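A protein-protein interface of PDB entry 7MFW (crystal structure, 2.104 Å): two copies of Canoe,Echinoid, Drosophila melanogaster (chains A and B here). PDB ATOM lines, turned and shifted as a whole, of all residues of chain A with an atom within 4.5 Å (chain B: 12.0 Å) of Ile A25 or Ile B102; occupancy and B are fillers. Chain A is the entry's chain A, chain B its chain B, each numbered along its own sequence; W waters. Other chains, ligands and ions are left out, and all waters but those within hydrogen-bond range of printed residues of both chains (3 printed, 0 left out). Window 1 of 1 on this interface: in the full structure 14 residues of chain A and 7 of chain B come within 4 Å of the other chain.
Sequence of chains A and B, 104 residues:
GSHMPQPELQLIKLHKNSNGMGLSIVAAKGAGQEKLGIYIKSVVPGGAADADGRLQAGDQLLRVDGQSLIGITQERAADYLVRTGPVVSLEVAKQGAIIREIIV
Water W1 bridges OE2 of Glu B101 and OG of Ser A24. Water W2 lies within hydrogen-bond range of the backbone carbonyl oxygen of Arg B100 (2.7 Å) and the backbone carbonyl oxygen of Ile A25 (3.2 Å). Water W3 lies within hydrogen-bond range of the backbone NH (N) of Ile B102 (2.7 Å), the backbone carbonyl oxygen (O) of Ile A25 (2.8 Å) and the side-chain hydroxyl (OG) of Ser A24 (2.8 Å).
Of chain B, only Ile B102 (3.7 Å), Ile B103 (3.5 Å) and Val B104 (2.9 Å) come within 4 Å of Leu A23. Of the printed residues of chain B, Ser A24 touches Glu B101 (3.99 Å), Ile B102 (3.3 Å) and Ile B103 (3.6 Å). Of chain B, only Ile B102 (2.9 Å) comes within 4 Å of Ile A25. No residue of chain B comes within 4 Å of Val A26. Ile A38 touches none of the printed residues of chain B. Of chain B, only Ile B102 comes within 4 Å of Gln A74. No residue of chain B comes within 4 Å of Ala A78. Of the printed residues of chain A, Glu B101 touches Ser A24. Ile B102 touches four residues of chain A. Of the printed residues of chain A, Ile B103 touches Leu A23 and Ser A24. The nearest residue of chain A that does not touch Ile B102 is Ala A78 (4.3 Å). The nearest printed residue of chain A that does not touch Ile B103 is Ile A25 (5.1 Å).
No position is printed for both chains.
O of Ser A24 sits at hydrogen-bond distance from N of Lys A41, 2.7 Å away.
Leu A23 touches Ile B102 (O to O, 3.7 Å). Leu A23 touches Ile B103. Glu B101 touches Ser A24. CA of Ser A24 touches O of Ile B102 (3.3 Å). Ser A24 touches Ile B103. Gln A74 touches Ile B102 (NE2 to CD1, 3.6 Å). Leu A81 touches Val B104.
N of Ile A25 lies within hydrogen-bond range of O of Ile B102 (2.9 Å). O of Leu A23 lies within hydrogen-bond range of N of Val B104, 2.9 Å away.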
ATOM      1  N   LEU A  23     -23.094  14.424 -29.990  1.00  0.00           N
ATOM      2  CA  LEU A  23     -22.003  14.984 -29.201  1.00  0.00           C
ATOM      3  C   LEU A  23     -22.472  15.359 -27.798  1.00  0.00           C
ATOM      4  O   LEU A  23     -23.485  16.044 -27.637  1.00  0.00           O
ATOM      5  CB  LEU A  23     -21.418  16.221 -29.893  1.00  0.00           C
ATOM      6  CG  LEU A  23     -20.655  16.033 -31.205  1.00  0.00           C
ATOM      7  CD1 LEU A  23     -20.260  17.375 -31.807  1.00  0.00           C
ATOM      8  CD2 LEU A  23     -19.427  15.172 -30.985  1.00  0.00           C
ATOM      9  N   SER A  24     -21.740  14.902 -26.787  1.00  0.00           N
ATOM     10  CA  SER A  24     -21.948  15.368 -25.419  1.00  0.00           C
ATOM     11  C   SER A  24     -20.938  16.480 -25.167  1.00  0.00           C
ATOM     12  O   SER A  24     -19.738  16.282 -25.359  1.00  0.00           O
ATOM     13  CB  SER A  24     -21.742  14.228 -24.421  1.00  0.00           C
ATOM     14  OG  SER A  24     -22.028  14.637 -23.096  1.00  0.00           O
ATOM     15  N   ILE A  25     -21.414  17.651 -24.758  1.00  0.00           N
ATOM     16  CA  ILE A  25     -20.535  18.811 -24.643  1.00  0.00           C
ATOM     17  C   ILE A  25     -20.433  19.374 -23.228  1.00  0.00           C
ATOM     18  O   ILE A  25     -21.311  19.158 -22.387  1.00  0.00           O
ATOM     19  CB  ILE A  25     -20.953  19.939 -25.607  1.00  0.00           C
ATOM     20  CG1 ILE A  25     -22.366  20.424 -25.278  1.00  0.00           C
ATOM     21  CG2 ILE A  25     -20.862  19.464 -27.056  1.00  0.00           C
ATOM     22  CD1 ILE A  25     -22.766  21.680 -26.013  1.00  0.00           C
ATOM     23  N   VAL A  26     -19.347  20.100 -22.983  1.00  0.00           N
ATOM     24  CA  VAL A  26     -19.090  20.717 -21.692  1.00  0.00           C
ATOM     25  C   VAL A  26     -18.420  22.072 -21.912  1.00  0.00           C
ATOM     26  O   VAL A  26     -17.586  22.225 -22.807  1.00  0.00           O
ATOM     27  CB  VAL A  26     -18.206  19.802 -20.803  1.00  0.00           C
ATOM     28  CG1 VAL A  26     -16.925  19.426 -21.524  1.00  0.00           C
ATOM     29  CG2 VAL A  26     -17.897  20.458 -19.469  1.00  0.00           C
ATOM     30  N   ILE A  38     -16.235  25.699 -25.616  1.00  0.00           N
ATOM     31  CA  ILE A  38     -17.091  24.520 -25.660  1.00  0.00           C
ATOM     32  C   ILE A  38     -16.283  23.307 -26.109  1.00  0.00           C
ATOM     33  O   ILE A  38     -15.668  23.322 -27.178  1.00  0.00           O
ATOM     34  CB  ILE A  38     -18.302  24.724 -26.586  1.00  0.00           C
ATOM     35  CG1 ILE A  38     -19.125  25.919 -26.112  1.00  0.00           C
ATOM     36  CG2 ILE A  38     -19.165  23.472 -26.613  1.00  0.00           C
ATOM     37  CD1 ILE A  38     -19.566  25.808 -24.665  1.00  0.00           C
ATOM     38  N   TYR A  39     -16.282  22.262 -25.287  1.00  0.00           N
ATOM     39  CA  TYR A  39     -15.473  21.081 -25.560  1.00  0.00           C
ATOM     40  C   TYR A  39     -16.317  19.823 -25.677  1.00  0.00           C
ATOM     41  O   TYR A  39     -17.380  19.709 -25.067  1.00  0.00           O
ATOM     42  CB  TYR A  39     -14.405  20.894 -24.479  1.00  0.00           C
ATOM     43  CG  TYR A  39     -13.409  22.026 -24.414  1.00  0.00           C
ATOM     44  CD1 TYR A  39     -12.208  21.960 -25.106  1.00  0.00           C
ATOM     45  CD2 TYR A  39     -13.676  23.166 -23.670  1.00  0.00           C
ATOM     46  CE1 TYR A  39     -11.299  22.994 -25.054  1.00  0.00           C
ATOM     47  CE2 TYR A  39     -12.773  24.204 -23.613  1.00  0.00           C
ATOM     48  CZ  TYR A  39     -11.588  24.113 -24.307  1.00  0.00           C
ATOM     49  OH  TYR A  39     -10.687  25.148 -24.252  1.00  0.00           O
ATOM     50  N   LYS A  41     -17.120  16.429 -24.563  1.00  0.00           N
ATOM     51  CA  LYS A  41     -16.921  15.539 -23.426  1.00  0.00           C
ATOM     52  C   LYS A  41     -16.839  14.112 -23.933  1.00  0.00           C
ATOM     53  O   LYS A  41     -15.932  13.362 -23.566  1.00  0.00           O
ATOM     54  CB  LYS A  41     -18.064  15.669 -22.416  1.00  0.00           C
ATOM     55  CG  LYS A  41     -18.011  14.639 -21.287  1.00  0.00           C
ATOM     56  CD  LYS A  41     -19.137  14.840 -20.284  1.00  0.00           C
ATOM     57  CE  LYS A  41     -18.792  14.225 -18.938  1.00  0.00           C
ATOM     58  NZ  LYS A  41     -17.502  14.755 -18.421  1.00  0.00           N
ATOM     59  N   LEU A  61     -14.931  23.039 -29.931  1.00  0.00           N
ATOM     60  CA  LEU A  61     -15.777  23.571 -30.989  1.00  0.00           C
ATOM     61  C   LEU A  61     -15.692  25.096 -30.976  1.00  0.00           C
ATOM     62  O   LEU A  61     -16.224  25.750 -30.077  1.00  0.00           O
ATOM     63  CB  LEU A  61     -17.223  23.112 -30.799  1.00  0.00           C
ATOM     64  CG  LEU A  61     -17.416  21.611 -30.573  1.00  0.00           C
ATOM     65  CD1 LEU A  61     -18.886  21.274 -30.406  1.00  0.00           C
ATOM     66  CD2 LEU A  61     -16.816  20.812 -31.713  1.00  0.00           C
ATOM     67  N   GLN A  74     -22.551  29.394 -21.215  1.00  0.00           N
ATOM     68  CA  GLN A  74     -22.900  28.024 -21.574  1.00  0.00           C
ATOM     69  C   GLN A  74     -24.261  27.930 -22.264  1.00  0.00           C
ATOM     70  O   GLN A  74     -24.413  27.209 -23.252  1.00  0.00           O
ATOM     71  CB  GLN A  74     -22.885  27.133 -20.330  1.00  0.00           C
ATOM     72  CG  GLN A  74     -23.445  25.736 -20.560  1.00  0.00           C
ATOM     73  CD  GLN A  74     -23.536  24.929 -19.281  1.00  0.00           C
ATOM     74  OE1 GLN A  74     -22.521  24.620 -18.658  1.00  0.00           O
ATOM     75  NE2 GLN A  74     -24.755  24.592 -18.880  1.00  0.00           N
ATOM     76  N   ALA A  78     -24.866  26.463 -26.087  1.00  0.00           N
ATOM     77  CA  ALA A  78     -25.701  25.280 -26.255  1.00  0.00           C
ATOM     78  C   ALA A  78     -26.891  25.567 -27.169  1.00  0.00           C
ATOM     79  O   ALA A  78     -27.318  24.702 -27.932  1.00  0.00           O
ATOM     80  CB  ALA A  78     -26.176  24.777 -24.908  1.00  0.00           C
ATOM     81  N   LEU A  81     -25.916  25.531 -30.823  1.00  0.00           N
ATOM     82  CA  LEU A  81     -25.638  24.172 -31.276  1.00  0.00           C
ATOM     83  C   LEU A  81     -26.909  23.361 -31.553  1.00  0.00           C
ATOM     84  O   LEU A  81     -26.942  22.552 -32.482  1.00  0.00           O
ATOM     85  CB  LEU A  81     -24.729  23.456 -30.269  1.00  0.00           C
ATOM     86  CG  LEU A  81     -23.261  23.891 -30.314  1.00  0.00           C
ATOM     87  CD1 LEU A  81     -22.521  23.545 -29.035  1.00  0.00           C
ATOM     88  CD2 LEU A  81     -22.564  23.256 -31.505  1.00  0.00           C
ATOM     89  N   ILE B  98     -23.360  19.670  -9.675  1.00  0.00           N
ATOM     90  CA  ILE B  98     -23.718  18.503 -10.468  1.00  0.00           C
ATOM     91  C   ILE B  98     -23.742  18.908 -11.940  1.00  0.00           C
ATOM     92  O   ILE B  98     -24.685  19.552 -12.399  1.00  0.00           O
ATOM     93  CB  ILE B  98     -25.096  17.937 -10.053  1.00  0.00           C
ATOM     94  CG1 ILE B  98     -25.039  17.382  -8.625  1.00  0.00           C
ATOM     95  CG2 ILE B  98     -25.557  16.867 -11.038  1.00  0.00           C
ATOM     96  CD1 ILE B  98     -26.398  17.045  -8.030  1.00  0.00           C
ATOM     97  N   ILE B  99     -22.692  18.543 -12.669  1.00  0.00           N
ATOM     98  CA  ILE B  99     -22.550  18.942 -14.067  1.00  0.00           C
ATOM     99  C   ILE B  99     -23.553  18.216 -14.964  1.00  0.00           C
ATOM    100  O   ILE B  99     -23.484  16.998 -15.134  1.00  0.00           O
ATOM    101  CB  ILE B  99     -21.110  18.718 -14.574  1.00  0.00           C
ATOM    102  CG1 ILE B  99     -20.136  19.605 -13.797  1.00  0.00           C
ATOM    103  CG2 ILE B  99     -21.009  19.013 -16.061  1.00  0.00           C
ATOM    104  CD1 ILE B  99     -20.437  21.086 -13.917  1.00  0.00           C
ATOM    105  N   ARG B 100     -24.481  18.982 -15.533  1.00  0.00           N
ATOM    106  CA  ARG B 100     -25.552  18.436 -16.359  1.00  0.00           C
ATOM    107  C   ARG B 100     -25.053  17.986 -17.728  1.00  0.00           C
ATOM    108  O   ARG B 100     -24.243  18.663 -18.362  1.00  0.00           O
ATOM    109  CB  ARG B 100     -26.670  19.468 -16.529  1.00  0.00           C
ATOM    110  CG  ARG B 100     -27.891  18.959 -17.287  1.00  0.00           C
ATOM    111  CD  ARG B 100     -28.952  20.043 -17.437  1.00  0.00           C
ATOM    112  NE  ARG B 100     -28.530  21.113 -18.339  1.00  0.00           N
ATOM    113  CZ  ARG B 100     -28.947  21.243 -19.595  1.00  0.00           C
ATOM    114  NH1 ARG B 100     -29.806  20.371 -20.106  1.00  0.00           N
ATOM    115  NH2 ARG B 100     -28.508  22.248 -20.341  1.00  0.00           N
ATOM    116  N   GLU B 101     -25.550  16.837 -18.175  1.00  0.00           N
ATOM    117  CA  GLU B 101     -25.222  16.299 -19.489  1.00  0.00           C
ATOM    118  C   GLU B 101     -25.911  17.097 -20.595  1.00  0.00           C
ATOM    119  O   GLU B 101     -27.141  17.162 -20.647  1.00  0.00           O
ATOM    120  CB  GLU B 101     -25.641  14.831 -19.567  1.00  0.00           C
ATOM    121  CG  GLU B 101     -25.301  14.145 -20.874  1.00  0.00           C
ATOM    122  CD  GLU B 101     -25.716  12.685 -20.893  1.00  0.00           C
ATOM    123  OE1 GLU B 101     -26.892  12.390 -20.581  1.00  0.00           O
ATOM    124  OE2 GLU B 101     -24.864  11.831 -21.218  1.00  0.00           O
ATOM    125  N   ILE B 102     -25.116  17.705 -21.470  1.00  0.00           N
ATOM    126  CA  ILE B 102     -25.648  18.450 -22.608  1.00  0.00           C
ATOM    127  C   ILE B 102     -25.388  17.700 -23.915  1.00  0.00           C
ATOM    128  O   ILE B 102     -24.241  17.554 -24.342  1.00  0.00           O
ATOM    129  CB  ILE B 102     -25.046  19.869 -22.690  1.00  0.00           C
ATOM    130  CG1 ILE B 102     -25.221  20.600 -21.357  1.00  0.00           C
ATOM    131  CG2 ILE B 102     -25.684  20.655 -23.827  1.00  0.00           C
ATOM    132  CD1 ILE B 102     -24.680  22.018 -21.352  1.00  0.00           C
ATOM    133  N   ILE B 103     -26.462  17.227 -24.541  1.00  0.00           N
ATOM    134  CA  ILE B 103     -26.366  16.447 -25.772  1.00  0.00           C
ATOM    135  C   ILE B 103     -26.870  17.257 -26.965  1.00  0.00           C
ATOM    136  O   ILE B 103     -27.950  17.847 -26.907  1.00  0.00           O
ATOM    137  CB  ILE B 103     -27.182  15.140 -25.669  1.00  0.00           C
ATOM    138  CG1 ILE B 103     -26.769  14.342 -24.429  1.00  0.00           C
ATOM    139  CG2 ILE B 103     -27.032  14.304 -26.936  1.00  0.00           C
ATOM    140  CD1 ILE B 103     -25.346  13.826 -24.475  1.00  0.00           C
ATOM    141  N   VAL B 104     -26.083  17.288 -28.040  1.00  0.00           N
ATOM    142  CA  VAL B 104     -26.472  17.983 -29.266  1.00  0.00           C
ATOM    143  C   VAL B 104     -26.222  17.098 -30.484  1.00  0.00           C
ATOM    144  O   VAL B 104     -25.668  16.003 -30.365  1.00  0.00           O
ATOM    145  CB  VAL B 104     -25.703  19.307 -29.446  1.00  0.00           C
ATOM    146  CG1 VAL B 104     -26.015  20.267 -28.315  1.00  0.00           C
ATOM    147  CG2 VAL B 104     -24.207  19.042 -29.525  1.00  0.00           C
ATOM    148  OXT VAL B 104     -26.562  17.455 -31.615  1.00  0.00           O
HETATM  149  O   HOH W   1     -22.397  12.669 -21.206  1.00  0.00           O
HETATM  150  O   HOH W   2     -22.085  19.861 -19.398  1.00  0.00           O
HETATM  151  O   HOH W   3     -22.528  16.854 -21.501  1.00  0.00           O
